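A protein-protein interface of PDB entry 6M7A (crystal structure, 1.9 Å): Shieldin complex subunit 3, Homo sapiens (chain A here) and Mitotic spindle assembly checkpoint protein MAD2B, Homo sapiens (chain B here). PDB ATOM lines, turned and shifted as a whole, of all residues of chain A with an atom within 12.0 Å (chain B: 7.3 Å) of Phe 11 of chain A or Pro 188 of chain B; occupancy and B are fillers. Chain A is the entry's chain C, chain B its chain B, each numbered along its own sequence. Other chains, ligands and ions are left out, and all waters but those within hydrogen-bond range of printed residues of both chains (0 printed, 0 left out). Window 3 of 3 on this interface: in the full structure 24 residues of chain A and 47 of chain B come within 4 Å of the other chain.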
ATOM      1  N   PHE A  11     -22.114 -30.722  -8.150  1.00  0.00           N
ATOM      2  CA  PHE A  11     -22.057 -30.200  -6.786  1.00  0.00           C
ATOM      3  C   PHE A  11     -23.021 -29.033  -6.617  1.00  0.00           C
ATOM      4  O   PHE A  11     -23.206 -28.236  -7.545  1.00  0.00           O
ATOM      5  CB  PHE A  11     -20.634 -29.755  -6.434  1.00  0.00           C
ATOM      6  CG  PHE A  11     -20.488 -29.236  -5.030  1.00  0.00           C
ATOM      7  CD1 PHE A  11     -20.464 -30.114  -3.958  1.00  0.00           C
ATOM      8  CD2 PHE A  11     -20.364 -27.874  -4.781  1.00  0.00           C
ATOM      9  CE1 PHE A  11     -20.323 -29.647  -2.657  1.00  0.00           C
ATOM     10  CE2 PHE A  11     -20.230 -27.395  -3.477  1.00  0.00           C
ATOM     11  CZ  PHE A  11     -20.208 -28.286  -2.416  1.00  0.00           C
ATOM     12  N   ILE A  12     -23.628 -28.930  -5.432  1.00  0.00           N
ATOM     13  CA  ILE A  12     -24.575 -27.869  -5.125  1.00  0.00           C
ATOM     14  C   ILE A  12     -24.288 -27.299  -3.740  1.00  0.00           C
ATOM     15  O   ILE A  12     -24.295 -28.039  -2.751  1.00  0.00           O
ATOM     16  CB  ILE A  12     -26.037 -28.348  -5.207  1.00  0.00           C
ATOM     17  CG1 ILE A  12     -26.312 -29.028  -6.550  1.00  0.00           C
ATOM     18  CG2 ILE A  12     -26.996 -27.180  -5.001  1.00  0.00           C
ATOM     19  CD1 ILE A  12     -26.307 -28.082  -7.737  1.00  0.00           C
ATOM     20  N   PRO A  13     -24.041 -25.995  -3.610  1.00  0.00           N
ATOM     21  CA  PRO A  13     -23.876 -25.405  -2.278  1.00  0.00           C
ATOM     22  C   PRO A  13     -25.200 -25.324  -1.540  1.00  0.00           C
ATOM     23  O   PRO A  13     -26.257 -25.108  -2.136  1.00  0.00           O
ATOM     24  CB  PRO A  13     -23.324 -24.000  -2.568  1.00  0.00           C
ATOM     25  CG  PRO A  13     -23.033 -23.964  -4.050  1.00  0.00           C
ATOM     26  CD  PRO A  13     -23.909 -24.992  -4.678  1.00  0.00           C
ATOM     27  N   TRP A  14     -25.131 -25.498  -0.220  1.00  0.00           N
ATOM     28  CA  TRP A  14     -26.330 -25.378   0.599  1.00  0.00           C
ATOM     29  C   TRP A  14     -26.818 -23.937   0.666  1.00  0.00           C
ATOM     30  O   TRP A  14     -28.029 -23.686   0.697  1.00  0.00           O
ATOM     31  CB  TRP A  14     -26.057 -25.905   2.005  1.00  0.00           C
ATOM     32  CG  TRP A  14     -25.581 -27.316   2.037  1.00  0.00           C
ATOM     33  CD1 TRP A  14     -25.674 -28.237   1.034  1.00  0.00           C
ATOM     34  CD2 TRP A  14     -24.927 -27.975   3.128  1.00  0.00           C
ATOM     35  NE1 TRP A  14     -25.117 -29.431   1.431  1.00  0.00           N
ATOM     36  CE2 TRP A  14     -24.648 -29.296   2.712  1.00  0.00           C
ATOM     37  CE3 TRP A  14     -24.542 -27.576   4.413  1.00  0.00           C
ATOM     38  CZ2 TRP A  14     -24.011 -30.220   3.540  1.00  0.00           C
ATOM     39  CZ3 TRP A  14     -23.915 -28.492   5.231  1.00  0.00           C
ATOM     40  CH2 TRP A  14     -23.649 -29.800   4.790  1.00  0.00           C
ATOM     41  N   PHE A  15     -25.897 -22.980   0.698  1.00  0.00           N
ATOM     42  CA  PHE A  15     -26.213 -21.570   0.929  1.00  0.00           C
ATOM     43  C   PHE A  15     -25.586 -20.727  -0.178  1.00  0.00           C
ATOM     44  O   PHE A  15     -24.535 -20.102   0.022  1.00  0.00           O
ATOM     45  CB  PHE A  15     -25.704 -21.115   2.301  1.00  0.00           C
ATOM     46  CG  PHE A  15     -26.207 -21.947   3.456  1.00  0.00           C
ATOM     47  CD1 PHE A  15     -27.547 -21.914   3.814  1.00  0.00           C
ATOM     48  CD2 PHE A  15     -25.341 -22.746   4.184  1.00  0.00           C
ATOM     49  CE1 PHE A  15     -28.017 -22.674   4.881  1.00  0.00           C
ATOM     50  CE2 PHE A  15     -25.801 -23.512   5.255  1.00  0.00           C
ATOM     51  CZ  PHE A  15     -27.141 -23.473   5.605  1.00  0.00           C
ATOM     52  N   PRO A  16     -26.206 -20.678  -1.355  1.00  0.00           N
ATOM     53  CA  PRO A  16     -25.633 -19.884  -2.452  1.00  0.00           C
ATOM     54  C   PRO A  16     -25.535 -18.409  -2.079  1.00  0.00           C
ATOM     55  O   PRO A  16     -26.285 -17.909  -1.237  1.00  0.00           O
ATOM     56  CB  PRO A  16     -26.621 -20.104  -3.601  1.00  0.00           C
ATOM     57  CG  PRO A  16     -27.921 -20.403  -2.915  1.00  0.00           C
ATOM     58  CD  PRO A  16     -27.572 -21.149  -1.656  1.00  0.00           C
ATOM     59  N   TYR A  17     -24.585 -17.716  -2.705  1.00  0.00           N
ATOM     60  CA  TYR A  17     -24.374 -16.299  -2.419  1.00  0.00           C
ATOM     61  C   TYR A  17     -25.673 -15.520  -2.583  1.00  0.00           C
ATOM     62  O   TYR A  17     -26.341 -15.594  -3.622  1.00  0.00           O
ATOM     63  CB  TYR A  17     -23.283 -15.713  -3.330  1.00  0.00           C
ATOM     64  CG  TYR A  17     -23.246 -14.194  -3.334  1.00  0.00           C
ATOM     65  CD1 TYR A  17     -24.045 -13.458  -4.214  1.00  0.00           C
ATOM     66  CD2 TYR A  17     -22.423 -13.495  -2.458  1.00  0.00           C
ATOM     67  CE1 TYR A  17     -24.032 -12.073  -4.209  1.00  0.00           C
ATOM     68  CE2 TYR A  17     -22.400 -12.104  -2.451  1.00  0.00           C
ATOM     69  CZ  TYR A  17     -23.204 -11.400  -3.328  1.00  0.00           C
ATOM     70  OH  TYR A  17     -23.179 -10.020  -3.329  1.00  0.00           O
ATOM     71  N   GLU B 101     -19.761 -24.344   4.990  1.00  0.00           N
ATOM     72  CA  GLU B 101     -21.208 -24.278   5.218  1.00  0.00           C
ATOM     73  C   GLU B 101     -21.571 -25.217   6.362  1.00  0.00           C
ATOM     74  O   GLU B 101     -21.109 -26.361   6.394  1.00  0.00           O
ATOM     75  CB  GLU B 101     -21.990 -24.660   3.963  1.00  0.00           C
ATOM     76  CG  GLU B 101     -21.558 -23.947   2.680  1.00  0.00           C
ATOM     77  CD  GLU B 101     -22.611 -24.041   1.586  1.00  0.00           C
ATOM     78  OE1 GLU B 101     -22.786 -25.150   1.041  1.00  0.00           O
ATOM     79  OE2 GLU B 101     -23.237 -23.013   1.248  1.00  0.00           O
ATOM     80  N   LYS B 129      -8.133 -32.843   3.318  1.00  0.00           N
ATOM     81  CA  LYS B 129      -8.480 -32.245   2.030  1.00  0.00           C
ATOM     82  C   LYS B 129      -7.827 -30.881   1.857  1.00  0.00           C
ATOM     83  O   LYS B 129      -7.327 -30.552   0.778  1.00  0.00           O
ATOM     84  CB  LYS B 129     -10.000 -32.111   1.893  1.00  0.00           C
ATOM     85  CG  LYS B 129     -10.710 -33.411   1.605  1.00  0.00           C
ATOM     86  CD  LYS B 129     -10.454 -33.842   0.181  1.00  0.00           C
ATOM     87  CE  LYS B 129     -11.100 -35.182  -0.101  1.00  0.00           C
ATOM     88  NZ  LYS B 129     -10.331 -36.261   0.571  1.00  0.00           N
ATOM     89  N   VAL B 136      -5.208 -28.873  -6.725  1.00  0.00           N
ATOM     90  CA  VAL B 136      -6.427 -28.697  -7.501  1.00  0.00           C
ATOM     91  C   VAL B 136      -6.819 -27.228  -7.642  1.00  0.00           C
ATOM     92  O   VAL B 136      -7.883 -26.925  -8.185  1.00  0.00           O
ATOM     93  CB  VAL B 136      -7.591 -29.517  -6.909  1.00  0.00           C
ATOM     94  CG1 VAL B 136      -7.222 -30.998  -6.865  1.00  0.00           C
ATOM     95  CG2 VAL B 136      -7.957 -29.005  -5.527  1.00  0.00           C
ATOM     96  N   ARG B 185     -15.513 -20.300 -10.103  1.00  0.00           N
ATOM     97  CA  ARG B 185     -15.436 -21.741 -10.254  1.00  0.00           C
ATOM     98  C   ARG B 185     -15.493 -22.371  -8.864  1.00  0.00           C
ATOM     99  O   ARG B 185     -14.795 -21.922  -7.949  1.00  0.00           O
ATOM    100  CB  ARG B 185     -14.149 -22.099 -10.996  1.00  0.00           C
ATOM    101  CG  ARG B 185     -13.670 -23.522 -10.877  1.00  0.00           C
ATOM    102  CD  ARG B 185     -12.443 -23.699 -11.763  1.00  0.00           C
ATOM    103  NE  ARG B 185     -11.490 -24.667 -11.228  1.00  0.00           N
ATOM    104  CZ  ARG B 185     -11.579 -25.982 -11.408  1.00  0.00           C
ATOM    105  NH1 ARG B 185     -10.665 -26.789 -10.880  1.00  0.00           N
ATOM    106  NH2 ARG B 185     -12.581 -26.490 -12.116  1.00  0.00           N
ATOM    107  N   LEU B 186     -16.362 -23.370  -8.689  1.00  0.00           N
ATOM    108  CA  LEU B 186     -16.551 -24.028  -7.398  1.00  0.00           C
ATOM    109  C   LEU B 186     -15.787 -25.348  -7.385  1.00  0.00           C
ATOM    110  O   LEU B 186     -15.988 -26.198  -8.263  1.00  0.00           O
ATOM    111  CB  LEU B 186     -18.035 -24.270  -7.117  1.00  0.00           C
ATOM    112  CG  LEU B 186     -19.021 -23.099  -7.009  1.00  0.00           C
ATOM    113  CD1 LEU B 186     -20.132 -23.471  -6.045  1.00  0.00           C
ATOM    114  CD2 LEU B 186     -18.357 -21.813  -6.554  1.00  0.00           C
ATOM    115  N   ILE B 187     -14.916 -25.517  -6.399  1.00  0.00           N
ATOM    116  CA  ILE B 187     -14.123 -26.727  -6.231  1.00  0.00           C
ATOM    117  C   ILE B 187     -14.517 -27.375  -4.910  1.00  0.00           C
ATOM    118  O   ILE B 187     -14.138 -26.907  -3.837  1.00  0.00           O
ATOM    119  CB  ILE B 187     -12.616 -26.422  -6.274  1.00  0.00           C
ATOM    120  CG1 ILE B 187     -12.252 -25.833  -7.639  1.00  0.00           C
ATOM    121  CG2 ILE B 187     -11.818 -27.688  -6.029  1.00  0.00           C
ATOM    122  CD1 ILE B 187     -11.500 -24.537  -7.561  1.00  0.00           C
ATOM    123  N   PRO B 188     -15.313 -28.439  -4.949  1.00  0.00           N
ATOM    124  CA  PRO B 188     -15.676 -29.132  -3.704  1.00  0.00           C
ATOM    125  C   PRO B 188     -14.461 -29.782  -3.066  1.00  0.00           C
ATOM    126  O   PRO B 188     -13.597 -30.331  -3.753  1.00  0.00           O
ATOM    127  CB  PRO B 188     -16.688 -30.190  -4.165  1.00  0.00           C
ATOM    128  CG  PRO B 188     -17.153 -29.732  -5.511  1.00  0.00           C
ATOM    129  CD  PRO B 188     -16.017 -28.980  -6.124  1.00  0.00           C
ATOM    130  N   LEU B 189     -14.408 -29.735  -1.736  1.00  0.00           N
ATOM    131  CA  LEU B 189     -13.348 -30.410  -1.000  1.00  0.00           C
ATOM    132  C   LEU B 189     -13.858 -31.567  -0.159  1.00  0.00           C
ATOM    133  O   LEU B 189     -13.323 -32.678  -0.246  1.00  0.00           O
ATOM    134  CB  LEU B 189     -12.598 -29.422  -0.098  1.00  0.00           C
ATOM    135  CG  LEU B 189     -11.789 -28.337  -0.817  1.00  0.00           C
ATOM    136  CD1 LEU B 189     -10.802 -27.688   0.176  1.00  0.00           C
ATOM    137  CD2 LEU B 189     -11.056 -28.929  -2.009  1.00  0.00           C
ATOM    138  N   LYS B 190     -14.885 -31.343   0.658  1.00  0.00           N
ATOM    139  CA  LYS B 190     -15.334 -32.393   1.559  1.00  0.00           C
ATOM    140  C   LYS B 190     -16.735 -32.065   2.067  1.00  0.00           C
ATOM    141  O   LYS B 190     -17.096 -30.895   2.192  1.00  0.00           O
ATOM    142  CB  LYS B 190     -14.346 -32.539   2.721  1.00  0.00           C
ATOM    143  CG  LYS B 190     -14.790 -33.464   3.832  1.00  0.00           C
ATOM    144  CD  LYS B 190     -15.139 -34.853   3.365  1.00  0.00           C
ATOM    145  CE  LYS B 190     -13.951 -35.624   2.856  1.00  0.00           C
ATOM    146  NZ  LYS B 190     -14.210 -37.086   3.045  1.00  0.00           N
ATOM    147  N   THR B 191     -17.516 -33.119   2.351  1.00  0.00           N
ATOM    148  CA  THR B 191     -18.819 -33.043   3.008  1.00  0.00           C
ATOM    149  C   THR B 191     -18.911 -34.114   4.092  1.00  0.00           C
ATOM    150  O   THR B 191     -18.382 -35.217   3.926  1.00  0.00           O
ATOM    151  CB  THR B 191     -19.961 -33.238   2.007  1.00  0.00           C
ATOM    152  OG1 THR B 191     -19.821 -32.295   0.936  1.00  0.00           O
ATOM    153  CG2 THR B 191     -21.314 -33.042   2.683  1.00  0.00           C
ATOM    154  N   GLN B 200     -20.052 -28.696   4.881  1.00  0.00           N
ATOM    155  CA  GLN B 200     -19.391 -28.948   3.614  1.00  0.00           C
ATOM    156  C   GLN B 200     -18.435 -27.807   3.330  1.00  0.00           C
ATOM    157  O   GLN B 200     -18.667 -26.662   3.724  1.00  0.00           O
ATOM    158  CB  GLN B 200     -20.394 -29.167   2.482  1.00  0.00           C
ATOM    159  CG  GLN B 200     -20.938 -27.951   1.815  1.00  0.00           C
ATOM    160  CD  GLN B 200     -21.968 -28.333   0.754  1.00  0.00           C
ATOM    161  OE1 GLN B 200     -22.064 -29.496   0.354  1.00  0.00           O
ATOM    162  NE2 GLN B 200     -22.748 -27.359   0.309  1.00  0.00           N
ATOM    163  N   LEU B 201     -17.329 -28.153   2.689  1.00  0.00           N
ATOM    164  CA  LEU B 201     -16.259 -27.210   2.409  1.00  0.00           C
ATOM    165  C   LEU B 201     -16.019 -27.201   0.913  1.00  0.00           C
ATOM    166  O   LEU B 201     -15.825 -28.260   0.308  1.00  0.00           O
ATOM    167  CB  LEU B 201     -14.976 -27.593   3.152  1.00  0.00           C
ATOM    168  CG  LEU B 201     -13.678 -26.927   2.697  1.00  0.00           C
ATOM    169  CD1 LEU B 201     -13.721 -25.449   2.946  1.00  0.00           C
ATOM    170  CD2 LEU B 201     -12.490 -27.576   3.450  1.00  0.00           C
ATOM    171  N   TYR B 202     -16.047 -26.016   0.317  1.00  0.00           N
ATOM    172  CA  TYR B 202     -15.682 -25.889  -1.079  1.00  0.00           C
ATOM    173  C   TYR B 202     -14.941 -24.576  -1.247  1.00  0.00           C
ATOM    174  O   TYR B 202     -14.986 -23.701  -0.372  1.00  0.00           O
ATOM    175  CB  TYR B 202     -16.910 -25.973  -1.992  1.00  0.00           C
ATOM    176  CG  TYR B 202     -17.987 -24.945  -1.734  1.00  0.00           C
ATOM    177  CD1 TYR B 202     -17.968 -23.706  -2.365  1.00  0.00           C
ATOM    178  CD2 TYR B 202     -19.055 -25.235  -0.890  1.00  0.00           C
ATOM    179  CE1 TYR B 202     -18.984 -22.773  -2.135  1.00  0.00           C
ATOM    180  CE2 TYR B 202     -20.058 -24.325  -0.660  1.00  0.00           C
ATOM    181  CZ  TYR B 202     -20.021 -23.101  -1.281  1.00  0.00           C
ATOM    182  OH  TYR B 202     -21.037 -22.217  -1.038  1.00  0.00           O
ATOM    183  N   VAL B 203     -14.222 -24.457  -2.362  1.00  0.00           N
ATOM    184  CA  VAL B 203     -13.441 -23.252  -2.664  1.00  0.00           C
ATOM    185  C   VAL B 203     -14.077 -22.565  -3.866  1.00  0.00           C
ATOM    186  O   VAL B 203     -14.471 -23.232  -4.838  1.00  0.00           O
ATOM    187  CB  VAL B 203     -11.959 -23.579  -2.932  1.00  0.00           C
ATOM    188  CG1 VAL B 203     -11.118 -22.290  -3.124  1.00  0.00           C
ATOM    189  CG2 VAL B 203     -11.360 -24.408  -1.812  1.00  0.00           C
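Of the 7 printed residues of chain A, 5 touch a printed residue of chain B. Hydrophobic or aromatic side chains of chain A within 4 Å of the printed part of chain B: Phe 11, Pro 13, Trp 14 and Phe 15. Along chain A the printed residues that touch a printed residue of chain B span positions 11 to 15. Among the printed residues, no Asp or Glu carboxylate lies within 4 Å of a Lys or Arg side-chain nitrogen of the other chain.
The backbone carbonyl oxygen of Gln 200 of chain B is in hydrogen-bond range of the backbone NH of Glu 101 of chain B, at 2.9 Å. The side-chain hydroxyl (OH) of Tyr 202 of chain B lies within hydrogen-bond range of the side-chain carboxylate (OE2) of Glu 101 of chain B, at 3.3 Å.
The side-chain carboxylate of Glu 101 of chain B lies within hydrogen-bond range of the backbone NH of Trp 14 of chain A, 2.7 Å away. The backbone NH (N) of Phe 15 of chain A lies within hydrogen-bond range of the side-chain carboxylate (OE2) of Glu 101 of chain B (2.7 Å). The side-chain amide nitrogen (NE2) of Gln 200 of chain B is in hydrogen-bond range of the backbone carbonyl oxygen (O) of Ile 12 of chain A (3.5 Å). The side-chain amide nitrogen (NE2) of Gln 200 of chain B lies close to the backbone NH (N) of Trp 14 of chain A (3.1 Å).
CG of Phe 11 of chain A touches CG of Pro 188 of chain B, 3.4 Å away. CE1 of Phe 11 of chain A touches OE1 of Gln 200 of chain B, 3.5 Å away. Phe 11 of chain A touches Tyr 202 of chain B. OE1 of Glu 101 of chain B touches CA of Pro 13 of chain A, at 3.5 Å. Pro 13 of chain A touches Leu 186 of chain B. Gln 200 of chain B touches Pro 13 of chain A. Tyr 202 of chain B touches Pro 13 of chain A (OH to CB, 3.3 Å). Trp 14 of chain A touches Thr 191 of chain B (CZ2 to CG2, 3.996 Å).
Phe 11 of chain A touches three residues of chain B. Of the printed residues of chain B, Trp 14 of chain A touches Glu 101 (2.7 Å), Thr 191 (3.996 Å) and Gln 200 (3.1 Å). Printed residues of chain B within 4 Å of Phe 15 of chain A: Glu 101 (2.7 Å). Pro 16 of chain A touches none of the printed residues of chain B. Of the printed residues of chain A, Glu 101 of chain B touches Pro 13 (3.5 Å), Trp 14 (2.7 Å) and Phe 15 (2.7 Å). Leu 186 of chain B touches just one residue of chain A: Pro 13 (3.6 Å). Pro 188 of chain B touches one residue of chain A. Leu 189 of chain B touches none of the printed residues of chain A. Printed residues of chain A within 4 Å of Thr 191 of chain B: Trp 14. Tyr 202 of chain B touches just these residues of chain A: Phe 11 (3.6 Å) and Pro 13 (3.3 Å). No residue of chain A comes within 4 Å of Val 203 of chain B. The nearest residue of chain B that does not touch Phe 11 of chain A is Thr 191 of chain B (4.5 Å).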
